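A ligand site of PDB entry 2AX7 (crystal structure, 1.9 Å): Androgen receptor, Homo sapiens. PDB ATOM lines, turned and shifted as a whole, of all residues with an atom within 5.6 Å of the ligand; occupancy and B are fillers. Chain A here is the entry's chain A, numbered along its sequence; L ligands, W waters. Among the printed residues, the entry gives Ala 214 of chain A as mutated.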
ATOM      1  N   LEU A  38      35.015  -3.343  24.580  1.00  0.00           N
ATOM      2  CA  LEU A  38      33.568  -3.270  24.719  1.00  0.00           C
ATOM      3  C   LEU A  38      33.043  -4.097  25.892  1.00  0.00           C
ATOM      4  O   LEU A  38      32.101  -3.681  26.574  1.00  0.00           O
ATOM      5  CB  LEU A  38      32.892  -3.682  23.404  1.00  0.00           C
ATOM      6  CG  LEU A  38      32.529  -2.488  22.512  1.00  0.00           C
ATOM      7  CD1 LEU A  38      31.467  -1.644  23.213  1.00  0.00           C
ATOM      8  CD2 LEU A  38      33.768  -1.641  22.222  1.00  0.00           C
ATOM      9  N   LEU A  41      33.571  -1.919  28.706  1.00  0.00           N
ATOM     10  CA  LEU A  41      32.663  -0.776  28.734  1.00  0.00           C
ATOM     11  C   LEU A  41      31.298  -1.260  29.244  1.00  0.00           C
ATOM     12  O   LEU A  41      30.626  -0.559  29.991  1.00  0.00           O
ATOM     13  CB  LEU A  41      32.502  -0.162  27.331  1.00  0.00           C
ATOM     14  CG  LEU A  41      33.591   0.802  26.850  1.00  0.00           C
ATOM     15  CD1 LEU A  41      33.276   1.238  25.427  1.00  0.00           C
ATOM     16  CD2 LEU A  41      33.660   2.016  27.766  1.00  0.00           C
ATOM     17  N   ASN A  42      30.903  -2.454  28.830  1.00  0.00           N
ATOM     18  CA  ASN A  42      29.624  -3.026  29.252  1.00  0.00           C
ATOM     19  C   ASN A  42      29.632  -3.305  30.760  1.00  0.00           C
ATOM     20  O   ASN A  42      28.688  -2.945  31.472  1.00  0.00           O
ATOM     21  CB  ASN A  42      29.314  -4.331  28.510  1.00  0.00           C
ATOM     22  CG  ASN A  42      29.002  -4.109  27.042  1.00  0.00           C
ATOM     23  OD1 ASN A  42      28.688  -2.990  26.621  1.00  0.00           O
ATOM     24  ND2 ASN A  42      29.079  -5.175  26.249  1.00  0.00           N
ATOM     25  N   GLU A  43      30.691  -3.945  31.237  1.00  0.00           N
ATOM     26  CA  GLU A  43      30.807  -4.252  32.663  1.00  0.00           C
ATOM     27  C   GLU A  43      30.825  -2.953  33.455  1.00  0.00           C
ATOM     28  O   GLU A  43      30.162  -2.836  34.484  1.00  0.00           O
ATOM     29  CB  GLU A  43      32.085  -5.058  32.936  1.00  0.00           C
ATOM     30  CG  GLU A  43      32.393  -5.258  34.412  1.00  0.00           C
ATOM     31  CD  GLU A  43      31.362  -6.114  35.135  1.00  0.00           C
ATOM     32  OE1 GLU A  43      31.278  -6.018  36.386  1.00  0.00           O
ATOM     33  OE2 GLU A  43      30.649  -6.894  34.466  1.00  0.00           O
ATOM     34  N   LEU A  44      31.592  -1.976  32.989  1.00  0.00           N
ATOM     35  CA  LEU A  44      31.670  -0.684  33.669  1.00  0.00           C
ATOM     36  C   LEU A  44      30.284  -0.053  33.709  1.00  0.00           C
ATOM     37  O   LEU A  44      29.863   0.474  34.740  1.00  0.00           O
ATOM     38  CB  LEU A  44      32.644   0.261  32.951  1.00  0.00           C
ATOM     39  CG  LEU A  44      32.777   1.668  33.565  1.00  0.00           C
ATOM     40  CD1 LEU A  44      33.205   1.582  35.020  1.00  0.00           C
ATOM     41  CD2 LEU A  44      33.790   2.482  32.770  1.00  0.00           C
ATOM     42  N   GLY A  45      29.579  -0.099  32.583  1.00  0.00           N
ATOM     43  CA  GLY A  45      28.245   0.475  32.510  1.00  0.00           C
ATOM     44  C   GLY A  45      27.362  -0.121  33.582  1.00  0.00           C
ATOM     45  O   GLY A  45      26.659   0.607  34.282  1.00  0.00           O
ATOM     46  N   GLN A  48      28.343   1.056  37.116  1.00  0.00           N
ATOM     47  CA  GLN A  48      27.893   2.425  37.348  1.00  0.00           C
ATOM     48  C   GLN A  48      26.377   2.478  37.554  1.00  0.00           C
ATOM     49  O   GLN A  48      25.893   3.295  38.331  1.00  0.00           O
ATOM     50  CB  GLN A  48      28.293   3.328  36.172  1.00  0.00           C
ATOM     51  CG  GLN A  48      29.810   3.438  36.016  1.00  0.00           C
ATOM     52  CD  GLN A  48      30.255   4.648  35.205  1.00  0.00           C
ATOM     53  OE1 GLN A  48      31.429   4.764  34.850  1.00  0.00           O
ATOM     54  NE2 GLN A  48      29.321   5.553  34.926  1.00  0.00           N
ATOM     55  N   GLN A  75      16.410   4.112  34.126  1.00  0.00           N
ATOM     56  CA  GLN A  75      16.833   3.326  32.972  1.00  0.00           C
ATOM     57  C   GLN A  75      16.973   4.139  31.680  1.00  0.00           C
ATOM     58  O   GLN A  75      17.881   3.881  30.890  1.00  0.00           O
ATOM     59  CB  GLN A  75      15.897   2.127  32.772  1.00  0.00           C
ATOM     60  CG  GLN A  75      15.916   1.166  33.973  1.00  0.00           C
ATOM     61  CD  GLN A  75      15.060  -0.073  33.784  1.00  0.00           C
ATOM     62  OE1 GLN A  75      14.126  -0.092  32.981  1.00  0.00           O
ATOM     63  NE2 GLN A  75      15.360  -1.118  34.548  1.00  0.00           N
ATOM     64  N   TRP A  78      19.996   6.738  32.280  1.00  0.00           N
ATOM     65  CA  TRP A  78      21.257   6.058  32.562  1.00  0.00           C
ATOM     66  C   TRP A  78      22.432   6.465  31.667  1.00  0.00           C
ATOM     67  O   TRP A  78      23.461   6.947  32.152  1.00  0.00           O
ATOM     68  CB  TRP A  78      21.013   4.542  32.506  1.00  0.00           C
ATOM     69  CG  TRP A  78      22.188   3.658  32.728  1.00  0.00           C
ATOM     70  CD1 TRP A  78      23.353   3.951  33.397  1.00  0.00           C
ATOM     71  CD2 TRP A  78      22.298   2.297  32.305  1.00  0.00           C
ATOM     72  NE1 TRP A  78      24.175   2.848  33.412  1.00  0.00           N
ATOM     73  CE2 TRP A  78      23.557   1.821  32.749  1.00  0.00           C
ATOM     74  CE3 TRP A  78      21.462   1.431  31.592  1.00  0.00           C
ATOM     75  CZ2 TRP A  78      23.992   0.513  32.502  1.00  0.00           C
ATOM     76  CZ3 TRP A  78      21.889   0.135  31.346  1.00  0.00           C
ATOM     77  CH2 TRP A  78      23.145  -0.309  31.796  1.00  0.00           C
ATOM     78  N   MET A  79      22.284   6.295  30.352  1.00  0.00           N
ATOM     79  CA  MET A  79      23.356   6.647  29.424  1.00  0.00           C
ATOM     80  C   MET A  79      23.758   8.124  29.541  1.00  0.00           C
ATOM     81  O   MET A  79      24.942   8.438  29.715  1.00  0.00           O
ATOM     82  CB  MET A  79      22.948   6.362  27.974  1.00  0.00           C
ATOM     83  CG  MET A  79      24.036   6.664  26.952  1.00  0.00           C
ATOM     84  SD  MET A  79      25.441   5.524  27.106  1.00  0.00           S
ATOM     85  CE  MET A  79      24.812   4.101  26.174  1.00  0.00           C
ATOM     86  N   MET A  82      25.684   8.995  32.661  1.00  0.00           N
ATOM     87  CA  MET A  82      27.071   8.541  32.584  1.00  0.00           C
ATOM     88  C   MET A  82      27.923   9.416  31.672  1.00  0.00           C
ATOM     89  O   MET A  82      29.080   9.689  31.998  1.00  0.00           O
ATOM     90  CB  MET A  82      27.135   7.092  32.094  1.00  0.00           C
ATOM     91  CG  MET A  82      26.617   6.043  33.063  1.00  0.00           C
ATOM     92  SD  MET A  82      27.279   4.395  32.677  1.00  0.00           S
ATOM     93  CE  MET A  82      26.402   4.022  31.155  1.00  0.00           C
ATOM     94  N   VAL A  83      27.371   9.821  30.539  1.00  0.00           N
ATOM     95  CA  VAL A  83      28.098  10.652  29.588  1.00  0.00           C
ATOM     96  C   VAL A  83      28.528  11.965  30.228  1.00  0.00           C
ATOM     97  O   VAL A  83      29.682  12.377  30.133  1.00  0.00           O
ATOM     98  CB  VAL A  83      27.230  10.996  28.352  1.00  0.00           C
ATOM     99  CG1 VAL A  83      27.910  12.080  27.517  1.00  0.00           C
ATOM    100  CG2 VAL A  83      27.026   9.741  27.506  1.00  0.00           C
ATOM    101  N   ALA A  85      28.803  12.731  33.439  1.00  0.00           N
ATOM    102  CA  ALA A  85      29.790  12.523  34.491  1.00  0.00           C
ATOM    103  C   ALA A  85      31.161  12.153  33.910  1.00  0.00           C
ATOM    104  O   ALA A  85      32.188  12.570  34.426  1.00  0.00           O
ATOM    105  CB  ALA A  85      29.318  11.438  35.462  1.00  0.00           C
ATOM    106  N   MET A  86      31.165  11.373  32.835  1.00  0.00           N
ATOM    107  CA  MET A  86      32.436  10.960  32.228  1.00  0.00           C
ATOM    108  C   MET A  86      33.160  12.177  31.646  1.00  0.00           C
ATOM    109  O   MET A  86      34.384  12.284  31.721  1.00  0.00           O
ATOM    110  CB  MET A  86      32.197   9.901  31.143  1.00  0.00           C
ATOM    111  CG  MET A  86      33.459   9.174  30.658  1.00  0.00           C
ATOM    112  SD  MET A  86      34.414  10.089  29.422  1.00  0.00           S
ATOM    113  CE  MET A  86      33.507   9.665  27.938  1.00  0.00           C
ATOM    114  N   ARG A  89      34.827  14.024  34.550  1.00  0.00           N
ATOM    115  CA  ARG A  89      36.013  13.318  35.028  1.00  0.00           C
ATOM    116  C   ARG A  89      37.165  13.531  34.063  1.00  0.00           C
ATOM    117  O   ARG A  89      38.316  13.696  34.469  1.00  0.00           O
ATOM    118  CB  ARG A  89      35.753  11.803  35.136  1.00  0.00           C
ATOM    119  CG  ARG A  89      34.851  11.388  36.284  1.00  0.00           C
ATOM    120  CD  ARG A  89      35.004   9.884  36.567  1.00  0.00           C
ATOM    121  NE  ARG A  89      34.591   9.044  35.442  1.00  0.00           N
ATOM    122  CZ  ARG A  89      33.324   8.769  35.140  1.00  0.00           C
ATOM    123  NH1 ARG A  89      32.337   9.262  35.878  1.00  0.00           N
ATOM    124  NH2 ARG A  89      33.043   7.990  34.102  1.00  0.00           N
ATOM    125  N   PHE A 101      36.859   7.081  31.282  1.00  0.00           N
ATOM    126  CA  PHE A 101      35.670   6.294  31.600  1.00  0.00           C
ATOM    127  C   PHE A 101      35.826   5.788  33.031  1.00  0.00           C
ATOM    128  O   PHE A 101      34.855   5.722  33.801  1.00  0.00           O
ATOM    129  CB  PHE A 101      35.511   5.097  30.657  1.00  0.00           C
ATOM    130  CG  PHE A 101      35.126   5.471  29.244  1.00  0.00           C
ATOM    131  CD1 PHE A 101      36.106   5.717  28.285  1.00  0.00           C
ATOM    132  CD2 PHE A 101      33.789   5.552  28.881  1.00  0.00           C
ATOM    133  CE1 PHE A 101      35.752   6.044  26.974  1.00  0.00           C
ATOM    134  CE2 PHE A 101      33.422   5.880  27.564  1.00  0.00           C
ATOM    135  CZ  PHE A 101      34.405   6.117  26.617  1.00  0.00           C
ATOM    136  N   MET A 117      33.502   3.430  18.343  1.00  0.00           N
ATOM    137  CA  MET A 117      32.611   4.463  18.900  1.00  0.00           C
ATOM    138  C   MET A 117      33.316   5.803  18.761  1.00  0.00           C
ATOM    139  O   MET A 117      33.122   6.695  19.584  1.00  0.00           O
ATOM    140  CB  MET A 117      32.353   4.212  20.382  1.00  0.00           C
ATOM    141  CG  MET A 117      31.897   2.816  20.725  1.00  0.00           C
ATOM    142  SD  MET A 117      31.924   2.596  22.516  1.00  0.00           S
ATOM    143  CE  MET A 117      30.421   3.346  22.957  1.00  0.00           C
ATOM    144  N   MET A 124      32.122  13.494  23.108  1.00  0.00           N
ATOM    145  CA  MET A 124      32.243  13.538  24.555  1.00  0.00           C
ATOM    146  C   MET A 124      33.531  14.268  24.944  1.00  0.00           C
ATOM    147  O   MET A 124      33.599  14.892  25.998  1.00  0.00           O
ATOM    148  CB  MET A 124      32.213  12.122  25.138  1.00  0.00           C
ATOM    149  CG  MET A 124      30.862  11.436  24.942  1.00  0.00           C
ATOM    150  SD  MET A 124      30.670   9.879  25.818  1.00  0.00           S
ATOM    151  CE  MET A 124      31.726   8.810  24.833  1.00  0.00           C
ATOM    152  N   LEU A 210      25.125   6.728  21.308  1.00  0.00           N
ATOM    153  CA  LEU A 210      25.638   5.608  22.089  1.00  0.00           C
ATOM    154  C   LEU A 210      24.552   4.552  22.234  1.00  0.00           C
ATOM    155  O   LEU A 210      24.831   3.360  22.179  1.00  0.00           O
ATOM    156  CB  LEU A 210      26.122   6.104  23.453  1.00  0.00           C
ATOM    157  CG  LEU A 210      27.414   6.922  23.437  1.00  0.00           C
ATOM    158  CD1 LEU A 210      27.616   7.611  24.767  1.00  0.00           C
ATOM    159  CD2 LEU A 210      28.595   6.019  23.109  1.00  0.00           C
ATOM    160  N   HIS A 211      23.306   4.985  22.406  1.00  0.00           N
ATOM    161  CA  HIS A 211      22.183   4.061  22.523  1.00  0.00           C
ATOM    162  C   HIS A 211      22.068   3.238  21.248  1.00  0.00           C
ATOM    163  O   HIS A 211      21.873   2.029  21.281  1.00  0.00           O
ATOM    164  CB  HIS A 211      20.871   4.818  22.744  1.00  0.00           C
ATOM    165  CG  HIS A 211      20.557   5.090  24.190  1.00  0.00           C
ATOM    166  ND1 HIS A 211      19.774   6.142  24.594  1.00  0.00           N
ATOM    167  CD2 HIS A 211      20.914   4.431  25.314  1.00  0.00           C
ATOM    168  CE1 HIS A 211      19.653   6.120  25.905  1.00  0.00           C
ATOM    169  NE2 HIS A 211      20.346   5.095  26.372  1.00  0.00           N
ATOM    170  N   PHE A 213      24.367   2.643  19.052  1.00  0.00           N
ATOM    171  CA  PHE A 213      25.541   1.783  18.963  1.00  0.00           C
ATOM    172  C   PHE A 213      25.370   0.539  19.830  1.00  0.00           C
ATOM    173  O   PHE A 213      25.578  -0.574  19.373  1.00  0.00           O
ATOM    174  CB  PHE A 213      26.794   2.554  19.389  1.00  0.00           C
ATOM    175  CG  PHE A 213      28.029   1.701  19.544  1.00  0.00           C
ATOM    176  CD1 PHE A 213      28.381   1.178  20.788  1.00  0.00           C
ATOM    177  CD2 PHE A 213      28.831   1.411  18.444  1.00  0.00           C
ATOM    178  CE1 PHE A 213      29.504   0.367  20.931  1.00  0.00           C
ATOM    179  CE2 PHE A 213      29.961   0.607  18.573  1.00  0.00           C
ATOM    180  CZ  PHE A 213      30.304   0.085  19.820  1.00  0.00           C
ATOM    181  N   ALA A 214      24.971   0.757  21.088  1.00  0.00           N
ATOM    182  CA  ALA A 214      24.782  -0.349  22.026  1.00  0.00           C
ATOM    183  C   ALA A 214      23.707  -1.309  21.529  1.00  0.00           C
ATOM    184  O   ALA A 214      23.818  -2.519  21.709  1.00  0.00           O
ATOM    185  CB  ALA A 214      24.392   0.197  23.404  1.00  0.00           C
ATOM    186  N   LEU A 217      25.085  -3.290  18.573  1.00  0.00           N
ATOM    187  CA  LEU A 217      26.087  -4.211  19.097  1.00  0.00           C
ATOM    188  C   LEU A 217      25.448  -5.410  19.777  1.00  0.00           C
ATOM    189  O   LEU A 217      25.892  -6.543  19.598  1.00  0.00           O
ATOM    190  CB  LEU A 217      27.019  -3.473  20.073  1.00  0.00           C
ATOM    191  CG  LEU A 217      28.187  -4.310  20.607  1.00  0.00           C
ATOM    192  CD1 LEU A 217      28.941  -4.944  19.444  1.00  0.00           C
ATOM    193  CD2 LEU A 217      29.116  -3.433  21.449  1.00  0.00           C
ATOM    194  N   PHE A 228      27.651  -9.065  27.245  1.00  0.00           N
ATOM    195  CA  PHE A 228      26.702  -8.100  27.788  1.00  0.00           C
ATOM    196  C   PHE A 228      26.136  -8.576  29.114  1.00  0.00           C
ATOM    197  O   PHE A 228      25.577  -9.668  29.203  1.00  0.00           O
ATOM    198  CB  PHE A 228      25.537  -7.863  26.830  1.00  0.00           C
ATOM    199  CG  PHE A 228      25.829  -6.846  25.757  1.00  0.00           C
ATOM    200  CD1 PHE A 228      26.320  -7.244  24.526  1.00  0.00           C
ATOM    201  CD2 PHE A 228      25.584  -5.494  25.979  1.00  0.00           C
ATOM    202  CE1 PHE A 228      26.577  -6.311  23.529  1.00  0.00           C
ATOM    203  CE2 PHE A 228      25.845  -4.550  24.989  1.00  0.00           C
ATOM    204  CZ  PHE A 228      26.345  -4.960  23.758  1.00  0.00           C
ATOM    205  N   MET A 232      22.019  -4.873  31.661  1.00  0.00           N
ATOM    206  CA  MET A 232      22.223  -4.050  30.474  1.00  0.00           C
ATOM    207  C   MET A 232      21.500  -4.633  29.251  1.00  0.00           C
ATOM    208  O   MET A 232      20.854  -3.900  28.503  1.00  0.00           O
ATOM    209  CB  MET A 232      23.714  -3.902  30.173  1.00  0.00           C
ATOM    210  CG  MET A 232      23.987  -3.009  28.964  1.00  0.00           C
ATOM    211  SD  MET A 232      25.743  -2.714  28.643  1.00  0.00           S
ATOM    212  CE  MET A 232      26.136  -1.584  29.998  1.00  0.00           C
ATOM    213  N   ILE A 235      17.788  -4.010  29.507  1.00  0.00           N
ATOM    214  CA  ILE A 235      17.488  -2.600  29.284  1.00  0.00           C
ATOM    215  C   ILE A 235      17.645  -2.180  27.820  1.00  0.00           C
ATOM    216  O   ILE A 235      16.849  -1.398  27.293  1.00  0.00           O
ATOM    217  CB  ILE A 235      18.365  -1.704  30.192  1.00  0.00           C
ATOM    218  CG1 ILE A 235      17.849  -1.796  31.638  1.00  0.00           C
ATOM    219  CG2 ILE A 235      18.363  -0.257  29.700  1.00  0.00           C
ATOM    220  CD1 ILE A 235      18.733  -1.124  32.670  1.00  0.00           C
ATOM    221  N   ILE A 236      18.695  -2.677  27.158  1.00  0.00           N
ATOM    222  CA  ILE A 236      18.919  -2.346  25.759  1.00  0.00           C
ATOM    223  C   ILE A 236      17.822  -2.913  24.874  1.00  0.00           C
ATOM    224  O   ILE A 236      17.448  -2.302  23.867  1.00  0.00           O
ATOM    225  CB  ILE A 236      20.268  -2.904  25.254  1.00  0.00           C
ATOM    226  CG1 ILE A 236      21.435  -2.230  25.986  1.00  0.00           C
ATOM    227  CG2 ILE A 236      20.394  -2.685  23.733  1.00  0.00           C
ATOM    228  CD1 ILE A 236      22.785  -2.827  25.656  1.00  0.00           C
ATOM    229  N   VAL A 240      15.690   0.885  25.649  1.00  0.00           N
ATOM    230  CA  VAL A 240      16.354   1.619  24.573  1.00  0.00           C
ATOM    231  C   VAL A 240      15.563   1.693  23.256  1.00  0.00           C
ATOM    232  O   VAL A 240      15.564   2.729  22.589  1.00  0.00           O
ATOM    233  CB  VAL A 240      17.758   1.055  24.295  1.00  0.00           C
ATOM    234  CG1 VAL A 240      18.375   1.726  23.063  1.00  0.00           C
ATOM    235  CG2 VAL A 240      18.651   1.299  25.513  1.00  0.00           C
HETATM  236  C1  LIG L   1      23.913   0.698  26.944  1.00  0.00           C
HETATM  237  C2  LIG L   1      22.593   1.127  27.046  1.00  0.00           C
HETATM  238  C3  LIG L   1      22.218   2.013  28.053  1.00  0.00           C
HETATM  239  F1  LIG L   1      20.938   2.427  28.155  1.00  0.00           F
HETATM  240  C4  LIG L   1      23.174   2.468  28.956  1.00  0.00           C
HETATM  241  C5  LIG L   1      24.494   2.038  28.855  1.00  0.00           C
HETATM  242  C6  LIG L   1      24.872   1.154  27.857  1.00  0.00           C
HETATM  243  O1  LIG L   1      26.169   0.738  27.814  1.00  0.00           O
HETATM  244  C7  LIG L   1      26.677   0.455  26.499  1.00  0.00           C
HETATM  245  C8  LIG L   1      28.198   0.480  26.555  1.00  0.00           C
HETATM  246  O2  LIG L   1      28.637  -0.522  27.480  1.00  0.00           O
HETATM  247  C9  LIG L   1      28.769   0.197  25.166  1.00  0.00           C
HETATM  248  C10 LIG L   1      28.650   1.856  27.052  1.00  0.00           C
HETATM  249  O3  LIG L   1      28.470   2.859  26.362  1.00  0.00           O
HETATM  250  N1  LIG L   1      29.227   1.848  28.246  1.00  0.00           N
HETATM  251  C11 LIG L   1      29.691   2.913  28.900  1.00  0.00           C
HETATM  252  C12 LIG L   1      29.538   4.221  28.444  1.00  0.00           C
HETATM  253  C13 LIG L   1      30.283   2.719  30.149  1.00  0.00           C
HETATM  254  C14 LIG L   1      30.685   3.809  30.903  1.00  0.00           C
HETATM  255  C15 LIG L   1      30.510   5.120  30.443  1.00  0.00           C
HETATM  256  N2  LIG L   1      30.891   6.084  31.275  1.00  0.00           N
HETATM  257  O4  LIG L   1      30.652   7.462  31.027  1.00  0.00           O
HETATM  258  O5  LIG L   1      31.469   5.749  32.527  1.00  0.00           O
HETATM  259  C16 LIG L   1      29.940   5.330  29.185  1.00  0.00           C
HETATM  260  C17 LIG L   1      29.731   6.742  28.584  1.00  0.00           C
HETATM  261  F2  LIG L   1      28.716   7.358  29.187  1.00  0.00           F
HETATM  262  F3  LIG L   1      30.818   7.507  28.693  1.00  0.00           F
HETATM  263  F4  LIG L   1      29.463   6.693  27.289  1.00  0.00           F
HETATM  264  O   HOH W   1      29.985   8.137  34.104  1.00  0.00           O
HETATM  265  O   HOH W   2      19.736   5.062  29.205  1.00  0.00           O
HETATM  266  O   HOH W   3      27.106   2.455  23.548  1.00  0.00           O
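O5 of the ligand sits close to OE1 of Gln 48, at 2.5 Å. The backbone NH of Asn 42 sits close to an oxygen (O2) of the ligand. The side-chain amide oxygen of Asn 42 sits at hydrogen-bond distance from an oxygen (O2) of the ligand (2.6 Å). The guanidinium group of Arg 89 sits at hydrogen-bond distance from an oxygen (O5) of the ligand (3.2 Å). The backbone carbonyl oxygen (O) of Leu 41 lies within hydrogen-bond range of an oxygen (O2) of the ligand (3.2 Å).
Water W2 lies within hydrogen-bond range of the backbone carbonyl oxygen (O) of Gln 75 (2.8 Å), a ring nitrogen (NE2) of His 211 (2.9 Å) and the backbone NH (N) of Met 79 (3.1 Å). Water W3 bridges O of Leu 210 (2.8 Å) and O3 of the ligand (3.2 Å). Water W1 lies within hydrogen-bond range of the backbone carbonyl oxygen (O) of Met 82 (2.8 Å), the side-chain amide nitrogen (NE2) of Gln 48 (2.8 Å), the guanidinium group (NH2) of Arg 89 (3.1 Å) and an oxygen (O4) of the ligand (3.2 Å).
The side-chain amide nitrogen (NE2) of Gln 48 is in hydrogen-bond range of the side-chain sulfur (SD) of Met 82 (3.3 Å). The side-chain amide oxygen of Asn 42 sits close to the side-chain sulfur of Met 232, at 3.6 Å. The backbone carbonyl oxygen (O) of Leu 38 lies close to the side-chain amide nitrogen (ND2) of Asn 42 (3.4 Å). SD of Met 82 sits close to NE1 of Trp 78, 3.5 Å away. O of Phe 101 lies within hydrogen-bond range of NH2 of Arg 89, at 2.9 Å. The backbone carbonyl oxygen (O) of Gly 45 lies close to the indole nitrogen (NE1) of Trp 78 (3.5 Å). The backbone NH (N) of Val 240 sits at hydrogen-bond distance from the backbone carbonyl oxygen (O) of Ile 235 (3.0 Å).
The backbone carbonyl oxygen (O) of Met 82 sits close to an oxygen (O4) of the ligand, at 2.9 Å. A fluorine (F2) of the ligand lies close to the backbone NH (N) of Val 83, at 3.1 Å. The side-chain sulfur (SD) of Met 124 sits close to a fluorine (F4) of the ligand. NE2 of His 211 sits close to F1 of the ligand (3.3 Å). The side-chain sulfur of Met 232 sits close to an oxygen (O1) of the ligand, at 3.6 Å. Merely in contact with the ligand: Met 86 (2.9 Å), Leu 210 (3.3 Å), Phe 101 (3.3 Å), Trp 78 (3.3 Å), Met 79 (3.4 Å), Ala 214 (3.6 Å), Val 240 (3.7 Å), Ile 236 (3.7 Å), Gly 45 (3.8 Å), Leu 38 (3.8 Å), Leu 44 (3.9 Å) and Met 117 (3.95 Å). Within 4 Å of the ligand: Leu 38, Leu 41, Asn 42, Leu 44, Gly 45, Gln 48, Trp 78, Met 79, Met 82, Val 83, Met 86, Arg 89, Phe 101, Met 117, Met 124, Leu 210, His 211, Ala 214, Met 232, Ile 236 and Val 240. Along chain A the residues within 4 Å of the ligand span positions 38 to 240. The nearest printed residue that does not touch the ligand is Ile 235 (4.03 Å).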
